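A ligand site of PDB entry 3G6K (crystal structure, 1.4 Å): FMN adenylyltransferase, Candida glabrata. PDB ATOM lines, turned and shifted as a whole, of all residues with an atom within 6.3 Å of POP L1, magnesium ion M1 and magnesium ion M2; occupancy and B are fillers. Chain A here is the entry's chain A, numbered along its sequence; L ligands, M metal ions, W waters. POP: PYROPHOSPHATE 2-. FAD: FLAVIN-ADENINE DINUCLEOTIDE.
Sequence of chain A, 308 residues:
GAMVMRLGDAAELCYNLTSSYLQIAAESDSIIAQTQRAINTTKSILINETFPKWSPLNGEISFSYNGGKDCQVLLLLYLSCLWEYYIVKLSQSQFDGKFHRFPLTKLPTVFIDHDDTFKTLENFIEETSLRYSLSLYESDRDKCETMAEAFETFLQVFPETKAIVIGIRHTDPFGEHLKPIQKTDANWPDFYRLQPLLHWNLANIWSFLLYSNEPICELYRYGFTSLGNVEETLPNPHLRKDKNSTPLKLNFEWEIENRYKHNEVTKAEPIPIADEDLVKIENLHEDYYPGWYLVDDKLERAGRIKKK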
ATOM      1  N   ASN A  66      21.746   0.206 -13.305  1.00  0.00           N
ATOM      2  CA  ASN A  66      20.350   0.603 -13.520  1.00  0.00           C
ATOM      3  C   ASN A  66      19.402  -0.228 -12.670  1.00  0.00           C
ATOM      4  O   ASN A  66      18.226  -0.294 -12.971  1.00  0.00           O
ATOM      5  CB  ASN A  66      19.928   0.502 -15.019  1.00  0.00           C
ATOM      6  CG  ASN A  66      19.779  -0.956 -15.469  1.00  0.00           C
ATOM      7  OD1 ASN A  66      20.213  -1.910 -14.809  1.00  0.00           O
ATOM      8  ND2 ASN A  66      19.137  -1.132 -16.605  1.00  0.00           N
ATOM      9  N   GLY A  67      19.896  -0.845 -11.608  1.00  0.00           N
ATOM     10  CA  GLY A  67      18.990  -1.551 -10.702  1.00  0.00           C
ATOM     11  C   GLY A  67      18.514  -2.927 -11.117  1.00  0.00           C
ATOM     12  O   GLY A  67      17.787  -3.566 -10.366  1.00  0.00           O
ATOM     13  N   GLY A  68      18.922  -3.368 -12.307  1.00  0.00           N
ATOM     14  CA  GLY A  68      18.503  -4.687 -12.716  1.00  0.00           C
ATOM     15  C   GLY A  68      19.294  -5.833 -12.090  1.00  0.00           C
ATOM     16  O   GLY A  68      20.264  -5.605 -11.356  1.00  0.00           O
ATOM     17  N   LYS A  69      18.852  -7.065 -12.373  1.00  0.00           N
ATOM     18  CA  LYS A  69      19.387  -8.221 -11.672  1.00  0.00           C
ATOM     19  C   LYS A  69      20.871  -8.466 -11.947  1.00  0.00           C
ATOM     20  O   LYS A  69      21.589  -8.982 -11.090  1.00  0.00           O
ATOM     21  CB  LYS A  69      18.568  -9.461 -12.062  1.00  0.00           C
ATOM     22  CG  LYS A  69      18.718  -9.807 -13.578  1.00  0.00           C
ATOM     23  CD  LYS A  69      17.673 -10.809 -14.054  1.00  0.00           C
ATOM     24  CE  LYS A  69      17.998 -11.349 -15.444  1.00  0.00           C
ATOM     25  NZ  LYS A  69      18.192 -10.251 -16.418  1.00  0.00           N
ATOM     26  N   ASP A  70      21.315  -8.125 -13.169  1.00  0.00           N
ATOM     27  CA  ASP A  70      22.679  -8.482 -13.572  1.00  0.00           C
ATOM     28  C   ASP A  70      23.643  -7.483 -13.021  1.00  0.00           C
ATOM     29  O   ASP A  70      24.649  -7.862 -12.399  1.00  0.00           O
ATOM     30  CB  ASP A  70      22.766  -8.536 -15.096  1.00  0.00           C
ATOM     31  CG  ASP A  70      21.761  -9.511 -15.669  1.00  0.00           C
ATOM     32  OD1 ASP A  70      21.839 -10.696 -15.319  1.00  0.00           O
ATOM     33  OD2 ASP A  70      20.838  -9.085 -16.414  1.00  0.00           O
ATOM     34  N   CYS A  71      23.355  -6.205 -13.171  1.00  0.00           N
ATOM     35  CA  CYS A  71      24.261  -5.250 -12.542  1.00  0.00           C
ATOM     36  C   CYS A  71      24.153  -5.277 -11.020  1.00  0.00           C
ATOM     37  O   CYS A  71      25.107  -4.964 -10.359  1.00  0.00           O
ATOM     38  CB  CYS A  71      24.131  -3.855 -13.108  1.00  0.00           C
ATOM     39  SG  CYS A  71      22.515  -3.099 -12.794  1.00  0.00           S
ATOM     40  N   GLN A  72      23.013  -5.692 -10.477  1.00  0.00           N
ATOM     41  CA  GLN A  72      22.943  -5.856  -9.019  1.00  0.00           C
ATOM     42  C   GLN A  72      23.831  -7.002  -8.536  1.00  0.00           C
ATOM     43  O   GLN A  72      24.605  -6.872  -7.585  1.00  0.00           O
ATOM     44  CB  GLN A  72      21.513  -6.056  -8.515  1.00  0.00           C
ATOM     45  CG  GLN A  72      21.462  -5.977  -6.981  1.00  0.00           C
ATOM     46  CD  GLN A  72      20.071  -6.159  -6.437  1.00  0.00           C
ATOM     47  OE1 GLN A  72      19.140  -6.539  -7.155  1.00  0.00           O
ATOM     48  NE2 GLN A  72      19.951  -5.956  -5.132  1.00  0.00           N
ATOM     49  N   GLY A 167      27.424  -4.731 -16.367  1.00  0.00           N
ATOM     50  CA  GLY A 167      26.934  -6.084 -16.021  1.00  0.00           C
ATOM     51  C   GLY A 167      26.361  -6.842 -17.235  1.00  0.00           C
ATOM     52  O   GLY A 167      25.409  -7.592 -17.109  1.00  0.00           O
ATOM     53  N   ILE A 168      26.978  -6.652 -18.396  1.00  0.00           N
ATOM     54  CA  ILE A 168      26.586  -7.317 -19.606  1.00  0.00           C
ATOM     55  C   ILE A 168      27.053  -8.763 -19.614  1.00  0.00           C
ATOM     56  O   ILE A 168      28.097  -9.101 -19.047  1.00  0.00           O
ATOM     57  CB  ILE A 168      27.122  -6.509 -20.834  1.00  0.00           C
ATOM     58  CG1 ILE A 168      26.520  -7.026 -22.127  1.00  0.00           C
ATOM     59  CG2 ILE A 168      28.643  -6.453 -20.872  1.00  0.00           C
ATOM     60  CD1 ILE A 168      26.482  -5.962 -23.214  1.00  0.00           C
ATOM     61  N   ARG A 169      26.262  -9.626 -20.260  1.00  0.00           N
ATOM     62  CA  ARG A 169      26.547 -11.044 -20.337  1.00  0.00           C
ATOM     63  C   ARG A 169      26.686 -11.456 -21.803  1.00  0.00           C
ATOM     64  O   ARG A 169      26.105 -10.780 -22.677  1.00  0.00           O
ATOM     65  CB  ARG A 169      25.429 -11.836 -19.642  1.00  0.00           C
ATOM     66  CG  ARG A 169      25.470 -11.553 -18.134  1.00  0.00           C
ATOM     67  CD  ARG A 169      24.135 -11.852 -17.400  1.00  0.00           C
ATOM     68  NE  ARG A 169      23.551 -13.098 -17.860  1.00  0.00           N
ATOM     69  CZ  ARG A 169      22.251 -13.302 -18.047  1.00  0.00           C
ATOM     70  NH1 ARG A 169      21.847 -14.389 -18.703  1.00  0.00           N
ATOM     71  NH2 ARG A 169      21.350 -12.434 -17.571  1.00  0.00           N
ATOM     72  N   ASP A 172      23.522 -11.589 -23.763  1.00  0.00           N
ATOM     73  CA  ASP A 172      22.794 -10.368 -24.113  1.00  0.00           C
ATOM     74  C   ASP A 172      23.026 -10.021 -25.588  1.00  0.00           C
ATOM     75  O   ASP A 172      24.003 -10.472 -26.201  1.00  0.00           O
ATOM     76  CB  ASP A 172      23.292  -9.223 -23.264  1.00  0.00           C
ATOM     77  CG  ASP A 172      22.895  -9.348 -21.807  1.00  0.00           C
ATOM     78  OD1 ASP A 172      21.845  -9.963 -21.521  1.00  0.00           O
ATOM     79  OD2 ASP A 172      23.606  -8.840 -20.935  1.00  0.00           O
ATOM     80  N   TYR A 220      10.668  -8.260 -11.110  1.00  0.00           N
ATOM     81  CA  TYR A 220      10.963  -9.653 -11.354  1.00  0.00           C
ATOM     82  C   TYR A 220       9.976 -10.551 -10.589  1.00  0.00           C
ATOM     83  O   TYR A 220       9.594 -11.595 -11.109  1.00  0.00           O
ATOM     84  CB  TYR A 220      12.416  -9.968 -10.951  1.00  0.00           C
ATOM     85  CG  TYR A 220      13.455  -9.183 -11.749  1.00  0.00           C
ATOM     86  CD1 TYR A 220      13.547  -9.317 -13.155  1.00  0.00           C
ATOM     87  CD2 TYR A 220      14.346  -8.351 -11.122  1.00  0.00           C
ATOM     88  CE1 TYR A 220      14.516  -8.614 -13.849  1.00  0.00           C
ATOM     89  CE2 TYR A 220      15.298  -7.628 -11.831  1.00  0.00           C
ATOM     90  CZ  TYR A 220      15.386  -7.792 -13.189  1.00  0.00           C
ATOM     91  OH  TYR A 220      16.368  -7.094 -13.845  1.00  0.00           O
ATOM     92  N   THR A 225      11.577 -10.895 -16.656  1.00  0.00           N
ATOM     93  CA  THR A 225      12.880 -11.544 -16.602  1.00  0.00           C
ATOM     94  C   THR A 225      13.969 -10.678 -17.204  1.00  0.00           C
ATOM     95  O   THR A 225      15.143 -11.057 -17.169  1.00  0.00           O
ATOM     96  CB  THR A 225      12.855 -12.883 -17.360  1.00  0.00           C
ATOM     97  OG1 THR A 225      12.410 -12.669 -18.716  1.00  0.00           O
ATOM     98  CG2 THR A 225      11.932 -13.872 -16.713  1.00  0.00           C
ATOM     99  N   SER A 226      13.560  -9.544 -17.776  1.00  0.00           N
ATOM    100  CA  SER A 226      14.454  -8.629 -18.487  1.00  0.00           C
ATOM    101  C   SER A 226      13.757  -7.317 -18.480  1.00  0.00           C
ATOM    102  O   SER A 226      12.589  -7.260 -18.855  1.00  0.00           O
ATOM    103  CB  SER A 226      14.658  -9.119 -19.930  1.00  0.00           C
ATOM    104  OG  SER A 226      15.309  -8.154 -20.711  1.00  0.00           O
ATOM    105  N   LEU A 227      14.428  -6.245 -18.071  1.00  0.00           N
ATOM    106  CA  LEU A 227      13.808  -4.961 -17.926  1.00  0.00           C
ATOM    107  C   LEU A 227      14.200  -4.008 -19.008  1.00  0.00           C
ATOM    108  O   LEU A 227      15.269  -3.347 -18.898  1.00  0.00           O
ATOM    109  CB  LEU A 227      14.151  -4.368 -16.563  1.00  0.00           C
ATOM    110  CG  LEU A 227      13.781  -5.305 -15.403  1.00  0.00           C
ATOM    111  CD1 LEU A 227      14.129  -4.576 -14.073  1.00  0.00           C
ATOM    112  CD2 LEU A 227      12.314  -5.702 -15.454  1.00  0.00           C
ATOM    113  N   GLY A 228      13.397  -3.906 -20.068  1.00  0.00           N
ATOM    114  CA  GLY A 228      13.608  -2.919 -21.068  1.00  0.00           C
ATOM    115  C   GLY A 228      12.763  -1.694 -20.701  1.00  0.00           C
ATOM    116  O   GLY A 228      12.495  -1.429 -19.526  1.00  0.00           O
ATOM    117  N   GLU A 300      15.155 -15.225 -22.209  1.00  0.00           N
ATOM    118  CA  GLU A 300      15.225 -14.126 -21.245  1.00  0.00           C
ATOM    119  C   GLU A 300      14.494 -12.875 -21.719  1.00  0.00           C
ATOM    120  O   GLU A 300      13.868 -12.178 -20.895  1.00  0.00           O
ATOM    121  CB  GLU A 300      16.694 -13.825 -20.887  1.00  0.00           C
ATOM    122  CG  GLU A 300      16.887 -12.762 -19.853  1.00  0.00           C
ATOM    123  CD  GLU A 300      18.343 -12.600 -19.414  1.00  0.00           C
ATOM    124  OE1 GLU A 300      19.148 -13.539 -19.659  1.00  0.00           O
ATOM    125  OE2 GLU A 300      18.671 -11.564 -18.836  1.00  0.00           O
ATOM    126  N   ARG A 301      14.590 -12.575 -23.024  1.00  0.00           N
ATOM    127  CA  ARG A 301      13.972 -11.388 -23.579  1.00  0.00           C
ATOM    128  C   ARG A 301      12.646 -11.645 -24.266  1.00  0.00           C
ATOM    129  O   ARG A 301      12.188 -10.807 -25.031  1.00  0.00           O
ATOM    130  CB  ARG A 301      14.906 -10.671 -24.567  1.00  0.00           C
ATOM    131  CG  ARG A 301      16.162 -10.159 -23.844  1.00  0.00           C
ATOM    132  CD  ARG A 301      17.230  -9.308 -24.607  1.00  0.00           C
ATOM    133  NE  ARG A 301      18.103  -8.373 -23.819  1.00  0.00           N
ATOM    134  CZ  ARG A 301      19.016  -8.682 -22.861  1.00  0.00           C
ATOM    135  NH1 ARG A 301      19.729  -7.735 -22.277  1.00  0.00           N
ATOM    136  NH2 ARG A 301      19.239  -9.914 -22.504  1.00  0.00           N
ATOM    137  N   ARG A 304       8.367  -9.172 -24.571  1.00  0.00           N
ATOM    138  CA  ARG A 304       8.418  -7.895 -25.312  1.00  0.00           C
ATOM    139  C   ARG A 304       7.198  -7.795 -26.213  1.00  0.00           C
ATOM    140  O   ARG A 304       6.707  -8.794 -26.747  1.00  0.00           O
ATOM    141  CB  ARG A 304       9.642  -7.820 -26.234  1.00  0.00           C
ATOM    142  CG  ARG A 304      10.990  -7.724 -25.561  1.00  0.00           C
ATOM    143  CD  ARG A 304      11.139  -6.435 -24.774  1.00  0.00           C
ATOM    144  NE  ARG A 304      12.486  -6.288 -24.219  1.00  0.00           N
ATOM    145  CZ  ARG A 304      12.897  -6.788 -23.083  1.00  0.00           C
ATOM    146  NH1 ARG A 304      12.070  -7.503 -22.310  1.00  0.00           N
ATOM    147  NH2 ARG A 304      14.143  -6.579 -22.697  1.00  0.00           N
HETATM  148  P1  POP L   1      18.002  -6.847 -17.033  1.00  0.00           P
HETATM  149  O1  POP L   1      16.975  -7.636 -16.320  1.00  0.00           O
HETATM  150  O2  POP L   1      18.876  -7.684 -17.916  1.00  0.00           O
HETATM  151  O3  POP L   1      17.368  -5.738 -17.778  1.00  0.00           O
HETATM  152  O   POP L   1      18.942  -6.193 -15.914  1.00  0.00           O
HETATM  153  P2  POP L   1      20.394  -5.505 -15.950  1.00  0.00           P
HETATM  154  O4  POP L   1      20.152  -4.033 -16.377  1.00  0.00           O
HETATM  155  O5  POP L   1      21.246  -6.158 -16.996  1.00  0.00           O
HETATM  156  O6  POP L   1      20.936  -5.545 -14.563  1.00  0.00           O
HETATM  157  PA  FAD L   2      20.852  -5.294 -20.070  1.00  0.00           P
HETATM  158  O1A FAD L   2      19.563  -4.615 -19.638  1.00  0.00           O
HETATM  159  O2A FAD L   2      21.021  -6.724 -19.789  1.00  0.00           O
HETATM  160  O5B FAD L   2      22.045  -4.375 -19.493  1.00  0.00           O
HETATM  161  C5B FAD L   2      23.378  -4.876 -19.529  1.00  0.00           C
HETATM  162  C4B FAD L   2      24.249  -3.964 -18.664  1.00  0.00           C
HETATM  163  O4B FAD L   2      24.354  -2.676 -19.228  1.00  0.00           O
HETATM  164  C3B FAD L   2      23.646  -3.699 -17.281  1.00  0.00           C
HETATM  165  O3B FAD L   2      23.885  -4.738 -16.347  1.00  0.00           O
HETATM  166  C2B FAD L   2      24.256  -2.400 -16.845  1.00  0.00           C
HETATM  167  O2B FAD L   2      25.606  -2.536 -16.323  1.00  0.00           O
HETATM  168  C1B FAD L   2      24.361  -1.663 -18.197  1.00  0.00           C
HETATM  169  N9A FAD L   2      23.194  -0.832 -18.445  1.00  0.00           N
HETATM  170  C8A FAD L   2      22.099  -1.088 -19.231  1.00  0.00           C
HETATM  171  N7A FAD L   2      21.296   0.004 -19.200  1.00  0.00           N
HETATM  172  C5A FAD L   2      21.850   0.943 -18.408  1.00  0.00           C
HETATM  173  C6A FAD L   2      21.478   2.218 -18.017  1.00  0.00           C
HETATM  174  N6A FAD L   2      20.345   2.799 -18.416  1.00  0.00           N
HETATM  175  N1A FAD L   2      22.328   2.907 -17.199  1.00  0.00           N
HETATM  176  C2A FAD L   2      23.484   2.350 -16.775  1.00  0.00           C
HETATM  177  N3A FAD L   2      23.877   1.106 -17.129  1.00  0.00           N
HETATM  178  C4A FAD L   2      23.048   0.426 -17.940  1.00  0.00           C
HETATM  179  N1  FAD L   2      28.080  -0.783 -26.899  1.00  0.00           N
HETATM  180  C2  FAD L   2      28.870  -0.772 -28.016  1.00  0.00           C
HETATM  181  O2  FAD L   2      28.483  -1.232 -29.100  1.00  0.00           O
HETATM  182  N3  FAD L   2      30.124  -0.273 -27.959  1.00  0.00           N
HETATM  183  C4  FAD L   2      30.642   0.272 -26.796  1.00  0.00           C
HETATM  184  O4  FAD L   2      31.793   0.745 -26.811  1.00  0.00           O
HETATM  185  C4X FAD L   2      29.834   0.280 -25.652  1.00  0.00           C
HETATM  186  N5  FAD L   2      30.312   0.856 -24.481  1.00  0.00           N
HETATM  187  C5X FAD L   2      29.463   0.831 -23.353  1.00  0.00           C
HETATM  188  C6  FAD L   2      29.924   1.376 -22.161  1.00  0.00           C
HETATM  189  C7  FAD L   2      29.088   1.402 -21.041  1.00  0.00           C
HETATM  190  C7M FAD L   2      29.595   1.973 -19.747  1.00  0.00           C
HETATM  191  C8  FAD L   2      27.792   0.863 -21.143  1.00  0.00           C
HETATM  192  C8M FAD L   2      26.855   0.862 -19.956  1.00  0.00           C
HETATM  193  C9  FAD L   2      27.336   0.325 -22.330  1.00  0.00           C
HETATM  194  C9A FAD L   2      28.174   0.292 -23.462  1.00  0.00           C
HETATM  195  N10 FAD L   2      27.725  -0.265 -24.644  1.00  0.00           N
HETATM  196  C10 FAD L   2      28.531  -0.210 -25.741  1.00  0.00           C
HETATM  197  C1' FAD L   2      26.306  -0.770 -24.733  1.00  0.00           C
HETATM  198  C2' FAD L   2      26.170  -2.114 -24.039  1.00  0.00           C
HETATM  199  O2' FAD L   2      26.976  -3.068 -24.725  1.00  0.00           O
HETATM  200  C3' FAD L   2      24.699  -2.569 -24.019  1.00  0.00           C
HETATM  201  O3' FAD L   2      24.271  -2.645 -25.369  1.00  0.00           O
HETATM  202  C4' FAD L   2      23.838  -1.543 -23.252  1.00  0.00           C
HETATM  203  O4' FAD L   2      24.328  -1.367 -21.926  1.00  0.00           O
HETATM  204  C5' FAD L   2      22.352  -1.895 -23.135  1.00  0.00           C
HETATM  205  O5' FAD L   2      22.300  -3.184 -22.535  1.00  0.00           O
HETATM  206  P   FAD L   2      20.997  -4.093 -22.731  1.00  0.00           P
HETATM  207  O1P FAD L   2      20.013  -3.191 -22.398  1.00  0.00           O
HETATM  208  O2P FAD L   2      20.928  -4.789 -24.070  1.00  0.00           O
HETATM  209  O3P FAD L   2      21.108  -5.228 -21.641  1.00  0.00           O
HETATM  210 MG    MG M   1      20.920  -7.856 -18.097  1.00  0.00          MG
HETATM  211 MG    MG M   2      17.569  -4.501 -19.473  1.00  0.00          MG
HETATM  212  O   HOH W   1      17.072  -5.548 -20.735  1.00  0.00           O
HETATM  213  O   HOH W   2      17.869  -2.650 -20.376  1.00  0.00           O
HETATM  214  O   HOH W   3      22.973  -8.267 -18.384  1.00  0.00           O
HETATM  215  O   HOH W   4      20.601  -9.531 -19.259  1.00  0.00           O
HETATM  216  O   HOH W   5      17.781  -3.084 -18.087  1.00  0.00           O
HETATM  217  O   HOH W   6      17.800  -8.687 -20.200  1.00  0.00           O
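Residues that only touch magnesium ion M1: Lys 69 (3.9996 Å). The nearest printed residue that does not touch magnesium ion M1 is Asp 172 (4.03 Å).
O6 of POP L1 sits close to O of Gly 68 (3.3 Å). Thr 225 touches POP L1 (O to O1, 3.97 Å). Ser 226 touches POP L1 (CA to O1, 3.5 Å). Glu 300 touches POP L1 (OE2 to O2, 3.99 Å). Hydrophobic or aromatic side chains that line POP L1: Tyr 220 and Leu 227. Of the 19 residues printed, 10 come within 4 Å of POP L1. Along chain A the residues within 4 Å of POP L1 span positions 66 to 300.
One residue has an atom within 4 Å of magnesium ion M2: Leu 227. The nearest printed residue that does not touch magnesium ion M2 is Gly 228 (4.3 Å).
Magnesium ion M2 is bound by water W1, water W5, O1A of FAD L2, water W2 and O3 of POP L1. Slightly farther from magnesium ion M2 lies the backbone carbonyl oxygen (O) of Leu 227 (2.6 Å).
The backbone NH (N) of Lys 69 sits at hydrogen-bond distance from an oxygen (O6) of POP L1 (3.4 Å). The backbone NH of Cys 71 is in hydrogen-bond range of an oxygen (O6) of POP L1 (2.9 Å). The side-chain amide oxygen of Asn 66 sits close to an oxygen (O4) of POP L1 (2.6 Å). An oxygen (O6) of POP L1 sits at hydrogen-bond distance from the side-chain sulfur (SG) of Cys 71 (3.4 Å). An oxygen (O3B) of FAD L2 lies within hydrogen-bond range of the backbone carbonyl oxygen (O) of Gly 167 (3.3 Å). An oxygen (O1) of POP L1 is in salt-bridge range of the side-chain amino group of Lys 69 (2.9 Å). O2B of FAD L2 lies within hydrogen-bond range of N of Gly 167, at 2.9 Å. An oxygen (O2P) of FAD L2 lies within salt-bridge range of the guanidinium group of Arg 301 (3.7 Å). N of Leu 227 lies within hydrogen-bond range of O1 of POP L1, at 3.4 Å. The backbone NH (N) of Asp 70 is in hydrogen-bond range of an oxygen (O6) of POP L1, 3.0 Å away. The side-chain hydroxyl of Tyr 220 is in hydrogen-bond range of an oxygen (O1) of POP L1 (2.6 Å).
Magnesium ion M1 is bound by O2A of FAD L2 (2.0 Å). An oxygen (O5) of POP L1 binds magnesium ion M1 (2.0 Å). Magnesium ion M1 is bound by O2 of POP L1. Magnesium ion M1 is bound by water W4, 2.1 Å away. Magnesium ion M1 is bound by OD2 of Asp 70 (2.1 Å). Water W3 is bound to magnesium ion M1. Magnesium ion M1 has six donor atoms within binding distance.
The side-chain carboxylate of Asp 70 is in salt-bridge range of the guanidinium group of Arg 169. OD1 of Asp 70 is in salt-bridge range of NZ of Lys 69. SG of Cys 71 is in hydrogen-bond range of N of Gly 67. OD1 of Asn 66 lies within hydrogen-bond range of SG of Cys 71. The backbone carbonyl oxygen (O) of Thr 225 sits at hydrogen-bond distance from the side-chain amino group (NZ) of Lys 69 (3.2 Å). The backbone NH of Gly 68 sits at hydrogen-bond distance from the side-chain amide oxygen of Asn 66. SG of Cys 71 is in hydrogen-bond range of N of Gly 68, at 3.6 Å. The side-chain carboxylate (OE1) of Glu 300 is in salt-bridge range of the guanidinium group (NH1) of Arg 169, 3.0 Å away.
Water W3 bridges the side-chain carboxylate (OD2) of Asp 172 (2.7 Å) and the backbone carbonyl oxygen (O) of Gly 167 (2.8 Å). Water W4 lies within hydrogen-bond range of OD1 of Asp 172, OE2 of Glu 300 and NH2 of Arg 169. Water W2 lies within hydrogen-bond range of O1P of FAD L2 (3.0 Å) and O of Leu 227 (3.1 Å). Water W1 bridges OG of Ser 226 (3.1 Å) and O of Leu 227 (3.4 Å). Water W5 lies within hydrogen-bond range of the backbone carbonyl oxygen of Leu 227 (2.7 Å), the side-chain amide nitrogen of Asn 66 (2.8 Å) and an oxygen (O4) of POP L1 (3.1 Å). Water W6 lies within hydrogen-bond range of OG of Ser 226 (2.6 Å), NH2 of Arg 301 (3.0 Å) and OE2 of Glu 300 (3.3 Å).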
